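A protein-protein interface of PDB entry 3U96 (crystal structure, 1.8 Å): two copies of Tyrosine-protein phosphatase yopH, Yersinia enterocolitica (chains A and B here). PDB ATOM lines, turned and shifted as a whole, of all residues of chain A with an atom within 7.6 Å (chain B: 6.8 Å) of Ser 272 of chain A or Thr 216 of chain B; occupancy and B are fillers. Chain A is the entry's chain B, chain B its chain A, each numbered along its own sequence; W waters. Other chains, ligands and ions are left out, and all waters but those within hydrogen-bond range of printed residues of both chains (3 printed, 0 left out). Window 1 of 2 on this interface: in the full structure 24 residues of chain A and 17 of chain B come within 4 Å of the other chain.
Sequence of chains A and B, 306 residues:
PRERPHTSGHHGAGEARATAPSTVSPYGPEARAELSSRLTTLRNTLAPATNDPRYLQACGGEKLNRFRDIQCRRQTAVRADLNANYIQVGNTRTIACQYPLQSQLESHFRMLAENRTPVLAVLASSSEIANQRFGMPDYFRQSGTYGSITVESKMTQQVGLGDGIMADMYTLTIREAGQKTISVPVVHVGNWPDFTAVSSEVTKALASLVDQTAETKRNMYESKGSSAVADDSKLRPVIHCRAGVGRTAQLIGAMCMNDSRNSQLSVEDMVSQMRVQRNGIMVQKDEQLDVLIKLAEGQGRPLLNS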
ATOM      1  N   LEU A  35      20.930 -13.392   7.798  1.00  0.00           N
ATOM      2  CA  LEU A  35      20.391 -14.497   6.998  1.00  0.00           C
ATOM      3  C   LEU A  35      18.935 -14.271   6.606  1.00  0.00           C
ATOM      4  O   LEU A  35      18.586 -14.372   5.411  1.00  0.00           O
ATOM      5  CB  LEU A  35      20.573 -15.828   7.722  1.00  0.00           C
ATOM      6  CG  LEU A  35      20.031 -17.077   7.016  1.00  0.00           C
ATOM      7  CD1 LEU A  35      20.711 -17.312   5.667  1.00  0.00           C
ATOM      8  CD2 LEU A  35      20.166 -18.298   7.898  1.00  0.00           C
ATOM      9  N   ARG A  38      18.578 -11.486   3.954  1.00  0.00           N
ATOM     10  CA  ARG A  38      18.975 -11.932   2.603  1.00  0.00           C
ATOM     11  C   ARG A  38      17.882 -12.843   2.024  1.00  0.00           C
ATOM     12  O   ARG A  38      17.488 -12.707   0.864  1.00  0.00           O
ATOM     13  CB  ARG A  38      20.300 -12.685   2.668  1.00  0.00           C
ATOM     14  CG  ARG A  38      21.471 -11.765   2.937  1.00  0.00           C
ATOM     15  CD  ARG A  38      22.805 -12.520   2.991  1.00  0.00           C
ATOM     16  NE  ARG A  38      23.825 -11.663   3.622  1.00  0.00           N
ATOM     17  CZ  ARG A  38      25.139 -11.893   3.609  1.00  0.00           C
ATOM     18  NH1 ARG A  38      25.627 -12.973   3.022  1.00  0.00           N
ATOM     19  NH2 ARG A  38      25.980 -11.038   4.203  1.00  0.00           N
ATOM     20  N   LEU A  39      17.371 -13.751   2.858  1.00  0.00           N
ATOM     21  CA  LEU A  39      16.347 -14.671   2.369  1.00  0.00           C
ATOM     22  C   LEU A  39      15.033 -13.959   2.013  1.00  0.00           C
ATOM     23  O   LEU A  39      14.342 -14.333   1.049  1.00  0.00           O
ATOM     24  CB  LEU A  39      16.140 -15.799   3.349  1.00  0.00           C
ATOM     25  CG  LEU A  39      17.358 -16.724   3.466  1.00  0.00           C
ATOM     26  CD1 LEU A  39      17.144 -17.770   4.542  1.00  0.00           C
ATOM     27  CD2 LEU A  39      17.678 -17.395   2.114  1.00  0.00           C
ATOM     28  N   LEU A  42      15.211 -12.305  -1.375  1.00  0.00           N
ATOM     29  CA  LEU A  42      15.106 -13.306  -2.419  1.00  0.00           C
ATOM     30  C   LEU A  42      13.668 -13.755  -2.645  1.00  0.00           C
ATOM     31  O   LEU A  42      13.202 -13.819  -3.794  1.00  0.00           O
ATOM     32  CB  LEU A  42      16.040 -14.494  -2.106  1.00  0.00           C
ATOM     33  CG  LEU A  42      16.068 -15.558  -3.206  1.00  0.00           C
ATOM     34  CD1 LEU A  42      16.591 -15.017  -4.569  1.00  0.00           C
ATOM     35  CD2 LEU A  42      16.928 -16.706  -2.716  1.00  0.00           C
ATOM     36  N   LEU A  46      11.604 -13.288  -6.139  1.00  0.00           N
ATOM     37  CA  LEU A  46      11.025 -14.479  -6.744  1.00  0.00           C
ATOM     38  C   LEU A  46       9.495 -14.526  -6.791  1.00  0.00           C
ATOM     39  O   LEU A  46       8.927 -15.478  -7.363  1.00  0.00           O
ATOM     40  CB  LEU A  46      11.558 -15.721  -6.025  1.00  0.00           C
ATOM     41  CG  LEU A  46      13.072 -15.916  -6.211  1.00  0.00           C
ATOM     42  CD1 LEU A  46      13.532 -17.156  -5.462  1.00  0.00           C
ATOM     43  CD2 LEU A  46      13.512 -15.966  -7.692  1.00  0.00           C
ATOM     44  N   GLN A  88      18.808 -29.132  -7.107  1.00  0.00           N
ATOM     45  CA  GLN A  88      20.110 -29.572  -6.642  1.00  0.00           C
ATOM     46  C   GLN A  88      20.642 -28.599  -5.631  1.00  0.00           C
ATOM     47  O   GLN A  88      20.788 -27.390  -5.913  1.00  0.00           O
ATOM     48  CB  GLN A  88      21.104 -29.723  -7.810  1.00  0.00           C
ATOM     49  CG  GLN A  88      22.456 -30.303  -7.395  1.00  0.00           C
ATOM     50  CD  GLN A  88      23.353 -30.541  -8.597  1.00  0.00           C
ATOM     51  OE1 GLN A  88      22.865 -30.840  -9.693  1.00  0.00           O
ATOM     52  NE2 GLN A  88      24.661 -30.410  -8.405  1.00  0.00           N
ATOM     53  N   VAL A  89      20.940 -29.119  -4.450  1.00  0.00           N
ATOM     54  CA  VAL A  89      21.450 -28.287  -3.366  1.00  0.00           C
ATOM     55  C   VAL A  89      22.867 -28.762  -3.090  1.00  0.00           C
ATOM     56  O   VAL A  89      23.077 -29.894  -2.606  1.00  0.00           O
ATOM     57  CB  VAL A  89      20.554 -28.381  -2.115  1.00  0.00           C
ATOM     58  CG1 VAL A  89      21.172 -27.639  -0.984  1.00  0.00           C
ATOM     59  CG2 VAL A  89      19.177 -27.782  -2.399  1.00  0.00           C
ATOM     60  N   SER A 266      26.761 -23.281   2.615  1.00  0.00           N
ATOM     61  CA  SER A 266      26.114 -22.559   3.706  1.00  0.00           C
ATOM     62  C   SER A 266      24.591 -22.714   3.745  1.00  0.00           C
ATOM     63  O   SER A 266      23.957 -23.107   2.767  1.00  0.00           O
ATOM     64  CB  SER A 266      26.469 -21.065   3.623  1.00  0.00           C
ATOM     65  OG  SER A 266      25.898 -20.484   2.448  1.00  0.00           O
ATOM     66  N   VAL A 267      23.987 -22.367   4.876  1.00  0.00           N
ATOM     67  CA  VAL A 267      22.527 -22.362   4.945  1.00  0.00           C
ATOM     68  C   VAL A 267      21.939 -21.350   3.922  1.00  0.00           C
ATOM     69  O   VAL A 267      20.936 -21.617   3.254  1.00  0.00           O
ATOM     70  CB  VAL A 267      22.081 -22.059   6.366  1.00  0.00           C
ATOM     71  CG1 VAL A 267      20.559 -21.866   6.439  1.00  0.00           C
ATOM     72  CG2 VAL A 267      22.528 -23.209   7.281  1.00  0.00           C
ATOM     73  N   GLU A 268      22.632 -20.195   3.828  1.00  0.00           N
ATOM     74  CA  GLU A 268      22.260 -19.199   2.817  1.00  0.00           C
ATOM     75  C   GLU A 268      22.264 -19.805   1.418  1.00  0.00           C
ATOM     76  O   GLU A 268      21.296 -19.623   0.675  1.00  0.00           O
ATOM     77  CB  GLU A 268      23.152 -17.935   2.869  1.00  0.00           C
ATOM     78  CG  GLU A 268      22.877 -16.949   1.716  1.00  0.00           C
ATOM     79  CD  GLU A 268      23.835 -15.720   1.692  1.00  0.00           C
ATOM     80  OE1 GLU A 268      24.643 -15.558   2.644  1.00  0.00           O
ATOM     81  OE2 GLU A 268      23.759 -14.933   0.711  1.00  0.00           O
ATOM     82  N   ASP A 269      23.322 -20.565   1.078  1.00  0.00           N
ATOM     83  CA  ASP A 269      23.371 -21.321  -0.204  1.00  0.00           C
ATOM     84  C   ASP A 269      22.209 -22.287  -0.378  1.00  0.00           C
ATOM     85  O   ASP A 269      21.567 -22.298  -1.436  1.00  0.00           O
ATOM     86  CB  ASP A 269      24.628 -22.183  -0.319  1.00  0.00           C
ATOM     87  CG  ASP A 269      25.865 -21.412  -0.671  1.00  0.00           C
ATOM     88  OD1 ASP A 269      25.774 -20.445  -1.455  1.00  0.00           O
ATOM     89  OD2 ASP A 269      26.948 -21.825  -0.179  1.00  0.00           O
ATOM     90  N   MET A 270      21.976 -23.135   0.629  1.00  0.00           N
ATOM     91  CA  MET A 270      20.988 -24.224   0.526  1.00  0.00           C
ATOM     92  C   MET A 270      19.625 -23.633   0.280  1.00  0.00           C
ATOM     93  O   MET A 270      18.878 -24.136  -0.567  1.00  0.00           O
ATOM     94  CB  MET A 270      20.780 -24.928   1.858  1.00  0.00           C
ATOM     95  CG  MET A 270      21.745 -25.915   2.248  1.00  0.00           C
ATOM     96  SD  MET A 270      21.172 -26.365   3.919  1.00  0.00           S
ATOM     97  CE  MET A 270      22.840 -26.496   4.458  1.00  0.00           C
ATOM     98  N   VAL A 271      19.267 -22.636   1.101  1.00  0.00           N
ATOM     99  CA  VAL A 271      17.919 -22.037   0.952  1.00  0.00           C
ATOM    100  C   VAL A 271      17.762 -21.232  -0.337  1.00  0.00           C
ATOM    101  O   VAL A 271      16.712 -21.308  -1.010  1.00  0.00           O
ATOM    102  CB  VAL A 271      17.451 -21.208   2.198  1.00  0.00           C
ATOM    103  CG1 VAL A 271      15.971 -20.802   2.047  1.00  0.00           C
ATOM    104  CG2 VAL A 271      17.614 -22.001   3.465  1.00  0.00           C
ATOM    105  N   SER A 272      18.783 -20.451  -0.691  1.00  0.00           N
ATOM    106  CA  SER A 272      18.768 -19.719  -1.961  1.00  0.00           C
ATOM    107  C   SER A 272      18.640 -20.673  -3.158  1.00  0.00           C
ATOM    108  O   SER A 272      17.876 -20.411  -4.078  1.00  0.00           O
ATOM    109  CB  SER A 272      19.985 -18.778  -2.087  1.00  0.00           C
ATOM    110  OG  SER A 272      20.141 -18.265  -3.414  1.00  0.00           O
ATOM    111  N   GLN A 273      19.365 -21.788  -3.123  1.00  0.00           N
ATOM    112  CA  GLN A 273      19.252 -22.816  -4.146  1.00  0.00           C
ATOM    113  C   GLN A 273      17.866 -23.424  -4.223  1.00  0.00           C
ATOM    114  O   GLN A 273      17.324 -23.551  -5.306  1.00  0.00           O
ATOM    115  CB  GLN A 273      20.321 -23.898  -3.974  1.00  0.00           C
ATOM    116  CG  GLN A 273      21.671 -23.365  -4.464  1.00  0.00           C
ATOM    117  CD  GLN A 273      22.853 -24.201  -4.024  1.00  0.00           C
ATOM    118  OE1 GLN A 273      22.715 -25.391  -3.797  1.00  0.00           O
ATOM    119  NE2 GLN A 273      24.021 -23.577  -3.899  1.00  0.00           N
ATOM    120  N   MET A 274      17.259 -23.730  -3.086  1.00  0.00           N
ATOM    121  CA  MET A 274      15.895 -24.282  -3.125  1.00  0.00           C
ATOM    122  C   MET A 274      14.903 -23.260  -3.694  1.00  0.00           C
ATOM    123  O   MET A 274      13.985 -23.630  -4.454  1.00  0.00           O
ATOM    124  CB  MET A 274      15.464 -24.762  -1.730  1.00  0.00           C
ATOM    125  CG  MET A 274      16.174 -26.049  -1.290  1.00  0.00           C
ATOM    126  SD  MET A 274      15.393 -26.696   0.257  1.00  0.00           S
ATOM    127  CE  MET A 274      16.377 -25.857   1.483  1.00  0.00           C
ATOM    128  N   ARG A 275      15.128 -21.990  -3.383  1.00  0.00           N
ATOM    129  CA  ARG A 275      14.203 -20.938  -3.809  1.00  0.00           C
ATOM    130  C   ARG A 275      14.255 -20.627  -5.277  1.00  0.00           C
ATOM    131  O   ARG A 275      13.212 -20.515  -5.926  1.00  0.00           O
ATOM    132  CB  ARG A 275      14.372 -19.663  -2.959  1.00  0.00           C
ATOM    133  CG  ARG A 275      13.774 -19.867  -1.557  1.00  0.00           C
ATOM    134  CD  ARG A 275      13.948 -18.684  -0.593  1.00  0.00           C
ATOM    135  NE  ARG A 275      13.217 -19.052   0.631  1.00  0.00           N
ATOM    136  CZ  ARG A 275      12.836 -18.217   1.589  1.00  0.00           C
ATOM    137  NH1 ARG A 275      13.090 -16.903   1.522  1.00  0.00           N
ATOM    138  NH2 ARG A 275      12.172 -18.709   2.620  1.00  0.00           N
ATOM    139  N   VAL A 276      15.472 -20.522  -5.801  1.00  0.00           N
ATOM    140  CA  VAL A 276      15.694 -20.248  -7.199  1.00  0.00           C
ATOM    141  C   VAL A 276      15.208 -21.402  -8.080  1.00  0.00           C
ATOM    142  O   VAL A 276      14.769 -21.184  -9.225  1.00  0.00           O
ATOM    143  CB  VAL A 276      17.181 -19.896  -7.414  1.00  0.00           C
ATOM    144  CG1 VAL A 276      17.573 -19.917  -8.877  1.00  0.00           C
ATOM    145  CG2 VAL A 276      17.461 -18.495  -6.815  1.00  0.00           C
ATOM    146  N   GLN A 277      15.240 -22.616  -7.533  1.00  0.00           N
ATOM    147  CA  GLN A 277      14.954 -23.797  -8.332  1.00  0.00           C
ATOM    148  C   GLN A 277      13.538 -24.330  -8.169  1.00  0.00           C
ATOM    149  O   GLN A 277      13.132 -25.258  -8.886  1.00  0.00           O
ATOM    150  CB  GLN A 277      15.972 -24.883  -8.019  1.00  0.00           C
ATOM    151  CG  GLN A 277      17.379 -24.559  -8.516  1.00  0.00           C
ATOM    152  CD  GLN A 277      18.361 -25.576  -8.009  1.00  0.00           C
ATOM    153  OE1 GLN A 277      18.255 -26.754  -8.349  1.00  0.00           O
ATOM    154  NE2 GLN A 277      19.300 -25.150  -7.174  1.00  0.00           N
ATOM    155  N   ARG A 278      12.779 -23.729  -7.263  1.00  0.00           N
ATOM    156  CA  ARG A 278      11.367 -24.086  -7.112  1.00  0.00           C
ATOM    157  C   ARG A 278      10.506 -22.831  -6.981  1.00  0.00           C
ATOM    158  O   ARG A 278       9.753 -22.490  -7.903  1.00  0.00           O
ATOM    159  CB  ARG A 278      11.168 -25.051  -5.921  1.00  0.00           C
ATOM    160  CG  ARG A 278       9.687 -25.380  -5.613  1.00  0.00           C
ATOM    161  CD  ARG A 278       9.487 -26.835  -5.121  1.00  0.00           C
ATOM    162  NE  ARG A 278       8.114 -27.014  -4.620  1.00  0.00           N
ATOM    163  CZ  ARG A 278       7.042 -27.165  -5.404  1.00  0.00           C
ATOM    164  NH1 ARG A 278       7.188 -27.155  -6.725  1.00  0.00           N
ATOM    165  NH2 ARG A 278       5.822 -27.291  -4.861  1.00  0.00           N
ATOM    166  N   ASN A 279      10.570 -22.178  -5.826  1.00  0.00           N
ATOM    167  CA  ASN A 279       9.913 -20.882  -5.632  1.00  0.00           C
ATOM    168  C   ASN A 279      10.396 -20.228  -4.351  1.00  0.00           C
ATOM    169  O   ASN A 279      11.078 -20.867  -3.538  1.00  0.00           O
ATOM    170  CB  ASN A 279       8.376 -21.015  -5.645  1.00  0.00           C
ATOM    171  CG  ASN A 279       7.846 -21.854  -4.490  1.00  0.00           C
ATOM    172  OD1 ASN A 279       8.178 -21.597  -3.335  1.00  0.00           O
ATOM    173  ND2 ASN A 279       7.031 -22.895  -4.800  1.00  0.00           N
ATOM    174  N   MET A 282      10.170 -21.746  -0.395  1.00  0.00           N
ATOM    175  CA  MET A 282      10.939 -22.873   0.152  1.00  0.00           C
ATOM    176  C   MET A 282      11.545 -22.489   1.497  1.00  0.00           C
ATOM    177  O   MET A 282      12.242 -21.480   1.625  1.00  0.00           O
ATOM    178  CB  MET A 282      12.028 -23.327  -0.831  1.00  0.00           C
ATOM    179  CG  MET A 282      11.448 -23.889  -2.141  1.00  0.00           C
ATOM    180  SD  MET A 282      10.474 -25.401  -1.935  1.00  0.00           S
ATOM    181  CE  MET A 282      11.784 -26.628  -1.702  1.00  0.00           C
ATOM    182  N   VAL A 283      11.262 -23.328   2.483  1.00  0.00           N
ATOM    183  CA  VAL A 283      11.461 -23.016   3.904  1.00  0.00           C
ATOM    184  C   VAL A 283      10.459 -21.931   4.285  1.00  0.00           C
ATOM    185  O   VAL A 283      10.748 -20.713   4.280  1.00  0.00           O
ATOM    186  CB  VAL A 283      12.922 -22.693   4.328  1.00  0.00           C
ATOM    187  CG1 VAL A 283      13.016 -22.767   5.876  1.00  0.00           C
ATOM    188  CG2 VAL A 283      13.955 -23.655   3.694  1.00  0.00           C
ATOM    189  N   ASN A 305      27.216 -16.622   3.549  1.00  0.00           N
ATOM    190  CA  ASN A 305      28.337 -16.458   2.638  1.00  0.00           C
ATOM    191  C   ASN A 305      29.083 -15.173   2.921  1.00  0.00           C
ATOM    192  O   ASN A 305      28.471 -14.141   3.232  1.00  0.00           O
ATOM    193  CB  ASN A 305      27.837 -16.443   1.182  1.00  0.00           C
ATOM    194  CG  ASN A 305      27.368 -17.813   0.714  1.00  0.00           C
ATOM    195  OD1 ASN A 305      26.718 -17.948  -0.343  1.00  0.00           O
ATOM    196  ND2 ASN A 305      27.688 -18.834   1.489  1.00  0.00           N
ATOM    197  N   PRO B 118      29.597 -11.076  -9.082  1.00  0.00           N
ATOM    198  CA  PRO B 118      28.813 -12.069  -8.344  1.00  0.00           C
ATOM    199  C   PRO B 118      29.320 -13.514  -8.526  1.00  0.00           C
ATOM    200  O   PRO B 118      28.916 -14.382  -7.766  1.00  0.00           O
ATOM    201  CB  PRO B 118      27.404 -11.928  -8.941  1.00  0.00           C
ATOM    202  CG  PRO B 118      27.628 -11.457 -10.326  1.00  0.00           C
ATOM    203  CD  PRO B 118      28.865 -10.564 -10.262  1.00  0.00           C
ATOM    204  N   ASP B 211      25.363 -19.696 -12.679  1.00  0.00           N
ATOM    205  CA  ASP B 211      24.187 -18.834 -12.557  1.00  0.00           C
ATOM    206  C   ASP B 211      23.643 -18.809 -11.126  1.00  0.00           C
ATOM    207  O   ASP B 211      23.212 -17.759 -10.633  1.00  0.00           O
ATOM    208  CB  ASP B 211      23.076 -19.298 -13.506  1.00  0.00           C
ATOM    209  CG  ASP B 211      23.269 -18.803 -14.911  1.00  0.00           C
ATOM    210  OD1 ASP B 211      24.055 -17.856 -15.132  1.00  0.00           O
ATOM    211  OD2 ASP B 211      22.585 -19.329 -15.817  1.00  0.00           O
ATOM    212  N   GLN B 212      23.611 -19.966 -10.477  1.00  0.00           N
ATOM    213  CA  GLN B 212      23.090 -20.073  -9.107  1.00  0.00           C
ATOM    214  C   GLN B 212      23.994 -19.311  -8.143  1.00  0.00           C
ATOM    215  O   GLN B 212      23.517 -18.586  -7.246  1.00  0.00           O
ATOM    216  CB  GLN B 212      23.003 -21.546  -8.672  1.00  0.00           C
ATOM    217  CG  GLN B 212      22.564 -21.707  -7.215  1.00  0.00           C
ATOM    218  CD  GLN B 212      21.115 -21.240  -6.980  1.00  0.00           C
ATOM    219  OE1 GLN B 212      20.170 -21.887  -7.451  1.00  0.00           O
ATOM    220  NE2 GLN B 212      20.941 -20.124  -6.234  1.00  0.00           N
ATOM    221  N   THR B 213      25.300 -19.445  -8.359  1.00  0.00           N
ATOM    222  CA  THR B 213      26.273 -18.743  -7.514  1.00  0.00           C
ATOM    223  C   THR B 213      26.121 -17.228  -7.642  1.00  0.00           C
ATOM    224  O   THR B 213      26.124 -16.534  -6.644  1.00  0.00           O
ATOM    225  CB  THR B 213      27.683 -19.187  -7.880  1.00  0.00           C
ATOM    226  OG1 THR B 213      27.756 -20.612  -7.729  1.00  0.00           O
ATOM    227  CG2 THR B 213      28.727 -18.544  -6.948  1.00  0.00           C
ATOM    228  N   ALA B 214      26.023 -16.741  -8.877  1.00  0.00           N
ATOM    229  CA  ALA B 214      25.763 -15.331  -9.169  1.00  0.00           C
ATOM    230  C   ALA B 214      24.461 -14.850  -8.535  1.00  0.00           C
ATOM    231  O   ALA B 214      24.425 -13.754  -7.958  1.00  0.00           O
ATOM    232  CB  ALA B 214      25.733 -15.085 -10.668  1.00  0.00           C
ATOM    233  N   GLU B 215      23.408 -15.650  -8.650  1.00  0.00           N
ATOM    234  CA  GLU B 215      22.108 -15.208  -8.141  1.00  0.00           C
ATOM    235  C   GLU B 215      22.140 -15.064  -6.620  1.00  0.00           C
ATOM    236  O   GLU B 215      21.625 -14.078  -6.070  1.00  0.00           O
ATOM    237  CB  GLU B 215      20.986 -16.145  -8.607  1.00  0.00           C
ATOM    238  CG  GLU B 215      19.573 -15.710  -8.147  1.00  0.00           C
ATOM    239  CD  GLU B 215      19.012 -14.435  -8.853  1.00  0.00           C
ATOM    240  OE1 GLU B 215      17.778 -14.229  -8.757  1.00  0.00           O
ATOM    241  OE2 GLU B 215      19.769 -13.646  -9.486  1.00  0.00           O
ATOM    242  N   THR B 216      22.756 -16.019  -5.933  1.00  0.00           N
ATOM    243  CA  THR B 216      22.910 -15.899  -4.477  1.00  0.00           C
ATOM    244  C   THR B 216      23.697 -14.610  -4.081  1.00  0.00           C
ATOM    245  O   THR B 216      23.291 -13.849  -3.169  1.00  0.00           O
ATOM    246  CB  THR B 216      23.614 -17.135  -3.880  1.00  0.00           C
ATOM    247  OG1 THR B 216      22.863 -18.319  -4.175  1.00  0.00           O
ATOM    248  CG2 THR B 216      23.707 -16.998  -2.355  1.00  0.00           C
ATOM    249  N   LYS B 217      24.823 -14.362  -4.752  1.00  0.00           N
ATOM    250  CA  LYS B 217      25.629 -13.180  -4.442  1.00  0.00           C
ATOM    251  C   LYS B 217      24.950 -11.865  -4.855  1.00  0.00           C
ATOM    252  O   LYS B 217      25.014 -10.860  -4.130  1.00  0.00           O
ATOM    253  CB  LYS B 217      27.043 -13.312  -5.093  1.00  0.00           C
ATOM    254  CG  LYS B 217      28.026 -12.224  -4.672  1.00  0.00           C
ATOM    255  CD  LYS B 217      28.389 -12.302  -3.188  1.00  0.00           C
ATOM    256  CE  LYS B 217      29.436 -11.271  -2.834  1.00  0.00           C
ATOM    257  NZ  LYS B 217      29.941 -11.522  -1.419  1.00  0.00           N
ATOM    258  N   ARG B 218      24.283 -11.864  -6.002  1.00  0.00           N
ATOM    259  CA  ARG B 218      23.624 -10.654  -6.476  1.00  0.00           C
ATOM    260  C   ARG B 218      22.505 -10.318  -5.487  1.00  0.00           C
ATOM    261  O   ARG B 218      22.265  -9.142  -5.176  1.00  0.00           O
ATOM    262  CB  ARG B 218      23.009 -10.857  -7.852  1.00  0.00           C
ATOM    263  CG  ARG B 218      22.407  -9.578  -8.379  1.00  0.00           C
ATOM    264  CD  ARG B 218      21.575  -9.743  -9.632  1.00  0.00           C
ATOM    265  NE  ARG B 218      20.815  -8.497  -9.843  1.00  0.00           N
ATOM    266  CZ  ARG B 218      21.128  -7.510 -10.687  1.00  0.00           C
ATOM    267  NH1 ARG B 218      22.191  -7.585 -11.488  1.00  0.00           N
ATOM    268  NH2 ARG B 218      20.339  -6.441 -10.751  1.00  0.00           N
ATOM    269  N   ASN B 219      21.825 -11.361  -5.020  1.00  0.00           N
ATOM    270  CA  ASN B 219      20.764 -11.176  -4.023  1.00  0.00           C
ATOM    271  C   ASN B 219      21.260 -10.476  -2.757  1.00  0.00           C
ATOM    272  O   ASN B 219      20.582  -9.593  -2.213  1.00  0.00           O
ATOM    273  CB  ASN B 219      20.099 -12.500  -3.667  1.00  0.00           C
ATOM    274  CG  ASN B 219      19.075 -12.335  -2.555  1.00  0.00           C
ATOM    275  OD1 ASN B 219      18.025 -11.744  -2.774  1.00  0.00           O
ATOM    276  ND2 ASN B 219      19.411 -12.781  -1.358  1.00  0.00           N
ATOM    277  N   MET B 220      22.436 -10.872  -2.295  1.00  0.00           N
ATOM    278  CA  MET B 220      23.019 -10.248  -1.122  1.00  0.00           C
ATOM    279  C   MET B 220      23.187  -8.749  -1.409  1.00  0.00           C
ATOM    280  O   MET B 220      22.788  -7.910  -0.582  1.00  0.00           O
ATOM    281  CB  MET B 220      24.355 -10.899  -0.788  1.00  0.00           C
ATOM    282  CG  MET B 220      25.067 -10.336   0.425  1.00  0.00           C
ATOM    283  SD  MET B 220      25.863  -8.767   0.101  1.00  0.00           S
ATOM    284  CE  MET B 220      27.136  -9.205  -1.103  1.00  0.00           C
ATOM    285  N   TYR B 221      23.741  -8.398  -2.579  1.00  0.00           N
ATOM    286  CA  TYR B 221      23.894  -6.957  -2.912  1.00  0.00           C
ATOM    287  C   TYR B 221      22.549  -6.217  -2.975  1.00  0.00           C
ATOM    288  O   TYR B 221      22.413  -5.096  -2.447  1.00  0.00           O
ATOM    289  CB  TYR B 221      24.625  -6.760  -4.232  1.00  0.00           C
ATOM    290  CG  TYR B 221      26.106  -7.015  -4.132  1.00  0.00           C
ATOM    291  CD1 TYR B 221      26.909  -6.207  -3.328  1.00  0.00           C
ATOM    292  CD2 TYR B 221      26.720  -8.049  -4.863  1.00  0.00           C
ATOM    293  CE1 TYR B 221      28.274  -6.421  -3.225  1.00  0.00           C
ATOM    294  CE2 TYR B 221      28.113  -8.261  -4.786  1.00  0.00           C
ATOM    295  CZ  TYR B 221      28.878  -7.425  -3.966  1.00  0.00           C
ATOM    296  OH  TYR B 221      30.239  -7.574  -3.832  1.00  0.00           O
HETATM  297  O   HOH W   1      24.439 -20.582  -3.963  1.00  0.00           O
HETATM  298  O   HOH W   2      28.228 -12.228   0.571  1.00  0.00           O
HETATM  299  O   HOH W   3      22.002 -14.131  -0.930  1.00  0.00           O
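The side-chain amide nitrogen (NE2) of Gln 212 of chain B lies within hydrogen-bond range of the side-chain hydroxyl (OG) of Ser 272 of chain A, at 3.5 Å.
OE1 of Gln 212 of chain B lies within hydrogen-bond range of NE2 of Gln 277 of chain A (3.4 Å).
OG of Ser 272 of chain A lies within hydrogen-bond range of OG1 of Thr 216 of chain B (2.8 Å).
ND2 of Asn 219 of chain B is in hydrogen-bond range of O of Arg 38 of chain A (2.9 Å).
OD1 of Asn 219 of chain B is in hydrogen-bond range of N of Leu 42 of chain A (3.2 Å).
The side-chain hydroxyl (OG1) of Thr 216 of chain B lies within hydrogen-bond range of the backbone carbonyl oxygen (O) of Gln 212 of chain B (3.2 Å).
The guanidinium group (NH1) of Arg 38 of chain A lies within salt-bridge range of the side-chain carboxylate (OE1) of Glu 268 of chain A.
The backbone carbonyl oxygen of Gln 88 of chain A sits close to the side-chain amide oxygen of Gln 273 of chain A, 3.5 Å away.
The side-chain hydroxyl (OG) of Ser 266 of chain A sits at hydrogen-bond distance from the side-chain amide nitrogen (ND2) of Asn 305 of chain A (2.6 Å).
The side-chain carboxylate (OE1) of Glu 268 of chain A is in hydrogen-bond range of the backbone NH (N) of Asn 305 of chain A (2.9 Å).
CZ of Arg 38 of chain A touches CG of Met 220 of chain B (3.5 Å).
Glu 268 of chain A touches Thr 216 of chain B.
Gln 212 of chain B touches Gln 273 of chain A.
CG1 of Val 276 of chain A touches OE1 of Gln 212 of chain B (3.6 Å).
Val 276 of chain A touches Glu 215 of chain B.
Thr 216 of chain B touches Asn 305 of chain A.
Of the printed residues of chain B, Ser 272 of chain A touches Gln 212 (3.5 Å) and Thr 216 (2.8 Å).
Of the printed residues of chain A, Asn 219 of chain B touches Arg 38 (2.9 Å) and Leu 42 (3.2 Å).
Of the printed residues of chain B, Asn 305 of chain A touches Thr 216 (3.7 Å).
Printed residues of chain A within 4 Å of Glu 215 of chain B: Val 276.
Printed residues of chain B within 4 Å of Glu 268 of chain A: Thr 216 (3.7 Å).
Thr 213 of chain B touches none of the printed residues of chain A.
The nearest printed residue of chain B that does not touch Ser 272 of chain A is Glu 215 of chain B (5.0 Å).
Of the 24 printed residues of chain A, 8 touch a printed residue of chain B.
Hydrophobic or aromatic side chains of chain B that line the printed part of chain A: Met 220.
Among the printed residues, 11 pairs touch across the chains.
Among the printed residues, no Asp or Glu carboxylate lies within 4 Å of a Lys or Arg side-chain nitrogen of the other chain.
No position is printed for both chains.
Of the 11 pairs that touch across the chains among the printed residues, none has its exchanged pair printed and touching as well.
Water W3 lies within hydrogen-bond range of OE2 of Glu 268 of chain A (2.5 Å), O of Thr 216 of chain B (2.6 Å) and ND2 of Asn 219 of chain B (3.0 Å).
Water W2 lies within hydrogen-bond range of NZ of Lys 217 of chain B (2.7 Å) and O of Asn 305 of chain A (3.3 Å).
Water W1 lies within hydrogen-bond range of OG1 of Thr 216 of chain B (2.8 Å), OD1 of Asp 269 of chain A (2.8 Å) and NE2 of Gln 273 of chain A (3.0 Å).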
